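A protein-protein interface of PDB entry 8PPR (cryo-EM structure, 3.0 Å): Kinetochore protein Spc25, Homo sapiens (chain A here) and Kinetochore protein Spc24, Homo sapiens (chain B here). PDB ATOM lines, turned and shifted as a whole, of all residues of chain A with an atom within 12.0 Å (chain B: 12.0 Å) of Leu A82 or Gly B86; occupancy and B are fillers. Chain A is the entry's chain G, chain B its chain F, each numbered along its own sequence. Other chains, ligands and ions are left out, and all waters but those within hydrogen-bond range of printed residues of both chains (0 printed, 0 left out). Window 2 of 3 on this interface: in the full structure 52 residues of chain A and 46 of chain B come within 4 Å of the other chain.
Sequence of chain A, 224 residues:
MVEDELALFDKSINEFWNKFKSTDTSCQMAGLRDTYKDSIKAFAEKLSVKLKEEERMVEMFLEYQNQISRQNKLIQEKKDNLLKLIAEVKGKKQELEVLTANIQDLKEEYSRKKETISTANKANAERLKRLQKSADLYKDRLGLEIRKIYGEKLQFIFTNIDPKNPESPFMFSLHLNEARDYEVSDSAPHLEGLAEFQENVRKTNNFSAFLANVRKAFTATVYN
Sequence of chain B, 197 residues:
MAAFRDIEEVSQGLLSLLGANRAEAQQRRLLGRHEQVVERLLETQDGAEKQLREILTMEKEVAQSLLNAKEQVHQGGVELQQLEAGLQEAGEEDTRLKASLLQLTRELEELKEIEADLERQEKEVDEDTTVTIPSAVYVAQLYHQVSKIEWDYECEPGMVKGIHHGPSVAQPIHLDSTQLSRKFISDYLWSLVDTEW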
ATOM      1  N   ASP A  80      19.624  32.737  -2.285  1.00  0.00           N
ATOM      2  CA  ASP A  80      19.652  32.723  -3.744  1.00  0.00           C
ATOM      3  C   ASP A  80      19.703  31.292  -4.270  1.00  0.00           C
ATOM      4  O   ASP A  80      18.716  30.557  -4.193  1.00  0.00           O
ATOM      5  CB  ASP A  80      20.849  33.522  -4.264  1.00  0.00           C
ATOM      6  CG  ASP A  80      20.821  34.971  -3.818  1.00  0.00           C
ATOM      7  OD1 ASP A  80      19.871  35.358  -3.106  1.00  0.00           O
ATOM      8  OD2 ASP A  80      21.750  35.723  -4.181  1.00  0.00           O
ATOM      9  N   ASN A  81      20.863  30.905  -4.807  1.00  0.00           N
ATOM     10  CA  ASN A  81      21.033  29.544  -5.308  1.00  0.00           C
ATOM     11  C   ASN A  81      20.883  28.525  -4.185  1.00  0.00           C
ATOM     12  O   ASN A  81      20.314  27.445  -4.384  1.00  0.00           O
ATOM     13  CB  ASN A  81      22.396  29.405  -5.985  1.00  0.00           C
ATOM     14  CG  ASN A  81      22.578  30.378  -7.134  1.00  0.00           C
ATOM     15  OD1 ASN A  81      21.679  31.157  -7.451  1.00  0.00           O
ATOM     16  ND2 ASN A  81      23.747  30.340  -7.762  1.00  0.00           N
ATOM     17  N   LEU A  82      21.393  28.854  -2.995  1.00  0.00           N
ATOM     18  CA  LEU A  82      21.206  27.983  -1.840  1.00  0.00           C
ATOM     19  C   LEU A  82      19.729  27.854  -1.487  1.00  0.00           C
ATOM     20  O   LEU A  82      19.263  26.772  -1.108  1.00  0.00           O
ATOM     21  CB  LEU A  82      22.001  28.523  -0.651  1.00  0.00           C
ATOM     22  CG  LEU A  82      23.517  28.667  -0.828  1.00  0.00           C
ATOM     23  CD1 LEU A  82      24.215  28.681   0.520  1.00  0.00           C
ATOM     24  CD2 LEU A  82      24.081  27.560  -1.706  1.00  0.00           C
ATOM     25  N   LEU A  83      18.980  28.954  -1.597  1.00  0.00           N
ATOM     26  CA  LEU A  83      17.543  28.906  -1.351  1.00  0.00           C
ATOM     27  C   LEU A  83      16.846  28.008  -2.368  1.00  0.00           C
ATOM     28  O   LEU A  83      15.952  27.229  -2.018  1.00  0.00           O
ATOM     29  CB  LEU A  83      16.967  30.325  -1.376  1.00  0.00           C
ATOM     30  CG  LEU A  83      15.509  30.578  -0.973  1.00  0.00           C
ATOM     31  CD1 LEU A  83      15.364  31.997  -0.447  1.00  0.00           C
ATOM     32  CD2 LEU A  83      14.546  30.355  -2.132  1.00  0.00           C
ATOM     33  N   LYS A  84      17.248  28.102  -3.637  1.00  0.00           N
ATOM     34  CA  LYS A  84      16.682  27.218  -4.653  1.00  0.00           C
ATOM     35  C   LYS A  84      16.990  25.758  -4.337  1.00  0.00           C
ATOM     36  O   LYS A  84      16.132  24.882  -4.489  1.00  0.00           O
ATOM     37  CB  LYS A  84      17.215  27.588  -6.037  1.00  0.00           C
ATOM     38  CG  LYS A  84      17.099  29.060  -6.386  1.00  0.00           C
ATOM     39  CD  LYS A  84      17.977  29.407  -7.576  1.00  0.00           C
ATOM     40  CE  LYS A  84      18.092  30.910  -7.759  1.00  0.00           C
ATOM     41  NZ  LYS A  84      16.759  31.553  -7.921  1.00  0.00           N
ATOM     42  N   LEU A  85      18.218  25.481  -3.896  1.00  0.00           N
ATOM     43  CA  LEU A  85      18.598  24.107  -3.581  1.00  0.00           C
ATOM     44  C   LEU A  85      17.801  23.562  -2.399  1.00  0.00           C
ATOM     45  O   LEU A  85      17.342  22.412  -2.426  1.00  0.00           O
ATOM     46  CB  LEU A  85      20.101  24.029  -3.312  1.00  0.00           C
ATOM     47  CG  LEU A  85      20.651  22.698  -2.796  1.00  0.00           C
ATOM     48  CD1 LEU A  85      20.450  21.601  -3.827  1.00  0.00           C
ATOM     49  CD2 LEU A  85      22.124  22.839  -2.459  1.00  0.00           C
ATOM     50  N   ILE A  86      17.623  24.368  -1.348  1.00  0.00           N
ATOM     51  CA  ILE A  86      16.863  23.893  -0.193  1.00  0.00           C
ATOM     52  C   ILE A  86      15.388  23.729  -0.551  1.00  0.00           C
ATOM     53  O   ILE A  86      14.712  22.822  -0.050  1.00  0.00           O
ATOM     54  CB  ILE A  86      17.070  24.811   1.030  1.00  0.00           C
ATOM     55  CG1 ILE A  86      16.529  26.217   0.782  1.00  0.00           C
ATOM     56  CG2 ILE A  86      18.543  24.866   1.410  1.00  0.00           C
ATOM     57  CD1 ILE A  86      16.439  27.066   2.033  1.00  0.00           C
ATOM     58  N   ALA A  87      14.864  24.584  -1.433  1.00  0.00           N
ATOM     59  CA  ALA A  87      13.504  24.386  -1.924  1.00  0.00           C
ATOM     60  C   ALA A  87      13.388  23.074  -2.697  1.00  0.00           C
ATOM     61  O   ALA A  87      12.402  22.338  -2.556  1.00  0.00           O
ATOM     62  CB  ALA A  87      13.083  25.571  -2.793  1.00  0.00           C
ATOM     63  N   GLU A  88      14.394  22.768  -3.520  1.00  0.00           N
ATOM     64  CA  GLU A  88      14.394  21.512  -4.266  1.00  0.00           C
ATOM     65  C   GLU A  88      14.398  20.315  -3.324  1.00  0.00           C
ATOM     66  O   GLU A  88      13.663  19.341  -3.532  1.00  0.00           O
ATOM     67  CB  GLU A  88      15.603  21.458  -5.204  1.00  0.00           C
ATOM     68  CG  GLU A  88      15.560  20.315  -6.210  1.00  0.00           C
ATOM     69  CD  GLU A  88      16.177  19.035  -5.670  1.00  0.00           C
ATOM     70  OE1 GLU A  88      17.095  19.126  -4.828  1.00  0.00           O
ATOM     71  OE2 GLU A  88      15.736  17.941  -6.079  1.00  0.00           O
ATOM     72  N   VAL A  89      15.225  20.369  -2.277  1.00  0.00           N
ATOM     73  CA  VAL A  89      15.297  19.240  -1.353  1.00  0.00           C
ATOM     74  C   VAL A  89      14.004  19.110  -0.553  1.00  0.00           C
ATOM     75  O   VAL A  89      13.575  17.998  -0.237  1.00  0.00           O
ATOM     76  CB  VAL A  89      16.539  19.334  -0.442  1.00  0.00           C
ATOM     77  CG1 VAL A  89      17.799  19.569  -1.267  1.00  0.00           C
ATOM     78  CG2 VAL A  89      16.376  20.396   0.631  1.00  0.00           C
ATOM     79  N   LYS A  90      13.358  20.233  -0.215  1.00  0.00           N
ATOM     80  CA  LYS A  90      12.067  20.163   0.472  1.00  0.00           C
ATOM     81  C   LYS A  90      11.006  19.506  -0.408  1.00  0.00           C
ATOM     82  O   LYS A  90      10.224  18.660   0.059  1.00  0.00           O
ATOM     83  CB  LYS A  90      11.623  21.564   0.898  1.00  0.00           C
ATOM     84  CG  LYS A  90      10.172  21.653   1.345  1.00  0.00           C
ATOM     85  CD  LYS A  90       9.753  23.098   1.585  1.00  0.00           C
ATOM     86  CE  LYS A  90      10.023  23.977   0.366  1.00  0.00           C
ATOM     87  NZ  LYS A  90       9.648  25.406   0.588  1.00  0.00           N
ATOM     88  N   GLY A  91      10.960  19.902  -1.683  1.00  0.00           N
ATOM     89  CA  GLY A  91      10.066  19.249  -2.624  1.00  0.00           C
ATOM     90  C   GLY A  91      10.318  17.758  -2.719  1.00  0.00           C
ATOM     91  O   GLY A  91       9.381  16.947  -2.667  1.00  0.00           O
ATOM     92  N   LYS A  93      11.632  15.954  -0.484  1.00  0.00           N
ATOM     93  CA  LYS A  93      11.188  15.397   0.794  1.00  0.00           C
ATOM     94  C   LYS A  93       9.725  15.002   0.754  1.00  0.00           C
ATOM     95  O   LYS A  93       9.381  13.833   0.979  1.00  0.00           O
ATOM     96  CB  LYS A  93      11.432  16.375   1.952  1.00  0.00           C
ATOM     97  CG  LYS A  93      12.876  16.486   2.410  1.00  0.00           C
ATOM     98  CD  LYS A  93      13.010  17.157   3.771  1.00  0.00           C
ATOM     99  CE  LYS A  93      12.805  18.648   3.681  1.00  0.00           C
ATOM    100  NZ  LYS A  93      13.952  19.245   2.949  1.00  0.00           N
ATOM    101  N   GLY B  86      24.128  27.263   3.461  1.00  0.00           N
ATOM    102  CA  GLY B  86      24.215  25.851   3.786  1.00  0.00           C
ATOM    103  C   GLY B  86      24.215  24.951   2.566  1.00  0.00           C
ATOM    104  O   GLY B  86      23.386  24.051   2.453  1.00  0.00           O
ATOM    105  N   LEU B  87      25.153  25.201   1.649  1.00  0.00           N
ATOM    106  CA  LEU B  87      25.270  24.371   0.453  1.00  0.00           C
ATOM    107  C   LEU B  87      25.571  22.922   0.815  1.00  0.00           C
ATOM    108  O   LEU B  87      24.900  21.997   0.342  1.00  0.00           O
ATOM    109  CB  LEU B  87      26.358  24.935  -0.464  1.00  0.00           C
ATOM    110  CG  LEU B  87      26.617  24.212  -1.789  1.00  0.00           C
ATOM    111  CD1 LEU B  87      25.409  24.283  -2.707  1.00  0.00           C
ATOM    112  CD2 LEU B  87      27.853  24.775  -2.477  1.00  0.00           C
ATOM    113  N   GLN B  88      26.584  22.707   1.659  1.00  0.00           N
ATOM    114  CA  GLN B  88      26.989  21.351   2.012  1.00  0.00           C
ATOM    115  C   GLN B  88      25.914  20.658   2.843  1.00  0.00           C
ATOM    116  O   GLN B  88      25.655  19.461   2.666  1.00  0.00           O
ATOM    117  CB  GLN B  88      28.329  21.400   2.753  1.00  0.00           C
ATOM    118  CG  GLN B  88      29.193  20.138   2.684  1.00  0.00           C
ATOM    119  CD  GLN B  88      28.622  18.938   3.414  1.00  0.00           C
ATOM    120  OE1 GLN B  88      27.833  19.074   4.349  1.00  0.00           O
ATOM    121  NE2 GLN B  88      29.041  17.749   2.996  1.00  0.00           N
ATOM    122  N   GLU B  89      25.286  21.393   3.764  1.00  0.00           N
ATOM    123  CA  GLU B  89      24.195  20.830   4.554  1.00  0.00           C
ATOM    124  C   GLU B  89      23.040  20.400   3.658  1.00  0.00           C
ATOM    125  O   GLU B  89      22.507  19.290   3.793  1.00  0.00           O
ATOM    126  CB  GLU B  89      23.730  21.853   5.593  1.00  0.00           C
ATOM    127  CG  GLU B  89      22.767  21.312   6.635  1.00  0.00           C
ATOM    128  CD  GLU B  89      21.318  21.389   6.192  1.00  0.00           C
ATOM    129  OE1 GLU B  89      20.982  22.295   5.400  1.00  0.00           O
ATOM    130  OE2 GLU B  89      20.518  20.540   6.635  1.00  0.00           O
ATOM    131  N   ALA B  90      22.647  21.272   2.725  1.00  0.00           N
ATOM    132  CA  ALA B  90      21.572  20.941   1.799  1.00  0.00           C
ATOM    133  C   ALA B  90      21.941  19.734   0.948  1.00  0.00           C
ATOM    134  O   ALA B  90      21.089  18.889   0.659  1.00  0.00           O
ATOM    135  CB  ALA B  90      21.250  22.149   0.920  1.00  0.00           C
ATOM    136  N   GLY B  91      23.210  19.633   0.545  1.00  0.00           N
ATOM    137  CA  GLY B  91      23.640  18.486  -0.242  1.00  0.00           C
ATOM    138  C   GLY B  91      23.581  17.177   0.523  1.00  0.00           C
ATOM    139  O   GLY B  91      23.119  16.154   0.003  1.00  0.00           O
ATOM    140  N   GLU B  92      24.071  17.180   1.766  1.00  0.00           N
ATOM    141  CA  GLU B  92      24.027  15.961   2.573  1.00  0.00           C
ATOM    142  C   GLU B  92      22.586  15.534   2.861  1.00  0.00           C
ATOM    143  O   GLU B  92      22.254  14.340   2.802  1.00  0.00           O
ATOM    144  CB  GLU B  92      24.822  16.160   3.863  1.00  0.00           C
ATOM    145  CG  GLU B  92      26.318  16.267   3.628  1.00  0.00           C
ATOM    146  CD  GLU B  92      26.933  14.967   3.144  1.00  0.00           C
ATOM    147  OE1 GLU B  92      26.470  13.888   3.573  1.00  0.00           O
ATOM    148  OE2 GLU B  92      27.872  15.017   2.318  1.00  0.00           O
ATOM    149  N   GLU B  93      21.710  16.501   3.152  1.00  0.00           N
ATOM    150  CA  GLU B  93      20.279  16.216   3.290  1.00  0.00           C
ATOM    151  C   GLU B  93      19.687  15.684   1.991  1.00  0.00           C
ATOM    152  O   GLU B  93      18.754  14.865   2.002  1.00  0.00           O
ATOM    153  CB  GLU B  93      19.516  17.474   3.704  1.00  0.00           C
ATOM    154  CG  GLU B  93      18.228  17.184   4.420  1.00  0.00           C
ATOM    155  CD  GLU B  93      17.079  17.073   3.430  1.00  0.00           C
ATOM    156  OE1 GLU B  93      17.115  17.771   2.395  1.00  0.00           O
ATOM    157  OE2 GLU B  93      16.127  16.310   3.695  1.00  0.00           O
ATOM    158  N   ASP B  94      20.176  16.183   0.855  1.00  0.00           N
ATOM    159  CA  ASP B  94      19.685  15.715  -0.437  1.00  0.00           C
ATOM    160  C   ASP B  94      20.047  14.254  -0.634  1.00  0.00           C
ATOM    161  O   ASP B  94      19.223  13.449  -1.082  1.00  0.00           O
ATOM    162  CB  ASP B  94      20.258  16.574  -1.573  1.00  0.00           C
ATOM    163  CG  ASP B  94      19.832  16.090  -2.940  1.00  0.00           C
ATOM    164  OD1 ASP B  94      18.603  16.001  -3.180  1.00  0.00           O
ATOM    165  OD2 ASP B  94      20.701  15.796  -3.793  1.00  0.00           O
ATOM    166  N   THR B  95      21.273  13.896  -0.257  1.00  0.00           N
ATOM    167  CA  THR B  95      21.698  12.502  -0.296  1.00  0.00           C
ATOM    168  C   THR B  95      20.825  11.641   0.602  1.00  0.00           C
ATOM    169  O   THR B  95      20.367  10.562   0.191  1.00  0.00           O
ATOM    170  CB  THR B  95      23.173  12.393   0.102  1.00  0.00           C
ATOM    171  OG1 THR B  95      23.351  12.960   1.407  1.00  0.00           O
ATOM    172  CG2 THR B  95      24.049  13.107  -0.905  1.00  0.00           C
ATOM    173  N   ARG B  96      20.562  12.112   1.829  1.00  0.00           N
ATOM    174  CA  ARG B  96      19.733  11.322   2.738  1.00  0.00           C
ATOM    175  C   ARG B  96      18.366  11.027   2.138  1.00  0.00           C
ATOM    176  O   ARG B  96      17.892   9.883   2.182  1.00  0.00           O
ATOM    177  CB  ARG B  96      19.564  12.013   4.091  1.00  0.00           C
ATOM    178  CG  ARG B  96      20.851  12.369   4.804  1.00  0.00           C
ATOM    179  CD  ARG B  96      21.568  11.099   5.253  1.00  0.00           C
ATOM    180  NE  ARG B  96      22.425  10.519   4.226  1.00  0.00           N
ATOM    181  CZ  ARG B  96      23.510  11.106   3.738  1.00  0.00           C
ATOM    182  NH1 ARG B  96      23.913  12.291   4.171  1.00  0.00           N
ATOM    183  NH2 ARG B  96      24.215  10.488   2.793  1.00  0.00           N
ATOM    184  N   LEU B  97      17.703  12.034   1.564  1.00  0.00           N
ATOM    185  CA  LEU B  97      16.341  11.760   1.097  1.00  0.00           C
ATOM    186  C   LEU B  97      16.322  10.985  -0.216  1.00  0.00           C
ATOM    187  O   LEU B  97      15.365  10.250  -0.484  1.00  0.00           O
ATOM    188  CB  LEU B  97      15.476  13.005   0.938  1.00  0.00           C
ATOM    189  CG  LEU B  97      15.597  14.037  -0.162  1.00  0.00           C
ATOM    190  CD1 LEU B  97      14.344  14.681  -0.019  1.00  0.00           C
ATOM    191  CD2 LEU B  97      16.528  15.133   0.096  1.00  0.00           C
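Asn A81 touches none of the printed residues of chain B.
Of chain B, only Gly B86 and Leu B87 come within 4 Å of Leu A82.
Leu A83 touches none of the printed residues of chain B.
No residue of chain B comes within 4 Å of Lys A84.
Of chain B, only Leu B87 (3.6 Å) and Ala B90 (3.6 Å) come within 4 Å of Leu A85.
Of chain B, only Ala B90 comes within 4 Å of Ile A86.
Printed residues of chain B within 4 Å of Val A89: Ala B90, Glu B93, Asp B94 and Leu B97.
Of chain A, only Leu A82 comes within 4 Å of Gly B86.
Of chain A, only Leu A82 (3.7 Å) and Leu A85 (3.6 Å) come within 4 Å of Leu B87.
Of the printed residues of chain A, Glu B93 touches Val A89 (3.2 Å) and Lys A93 (3.2 Å).
Of the printed residues of chain A, Asp B94 touches Glu A88 and Val A89.
The nearest residue of chain B that does not touch Leu A82 is Ala B90 (5.4 Å).
The backbone carbonyl oxygen of Val A89 lies close to the side-chain amino group of Lys A93 (3.4 Å).
Leu A82 touches Gly B86 (CD1 to N, 3.3 Å).
Leu A82 touches Leu B87.
Leu A85 touches Leu B87 (CD2 to CD1, 3.6 Å).
Ala B90 touches Leu A85.
Ile A86 touches Ala B90.
OD1 of Asp B94 touches OE1 of Glu A88 (3.8 Å).
Ala B90 touches Val A89.
Glu B93 touches Val A89 (OE1 to CG2, 3.2 Å).
CD1 of Leu B97 touches O of Val A89, 3.4 Å away.
N of Lys A93 touches CD1 of Leu B97, 3.0 Å away.
The side-chain carboxylate (OE1) of Glu B93 lies within salt-bridge range of the side-chain amino group (NZ) of Lys A93 (3.5 Å).
Hydrophobic or aromatic side chains of chain B that line the printed part of chain A: Leu B87, Ala B90 and Leu B97.
Along chain B the printed residues that touch a printed residue of chain A span positions 86 to 97.
Hydrophobic or aromatic side chains of chain A that line the printed part of chain B: Leu A82, Leu A85, Ile A86 and Val A89.
Among the printed residues, Asp or Glu carboxylates within 4 Å of a Lys or Arg side-chain nitrogen of the other chain: Lys A93 with Glu B93.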
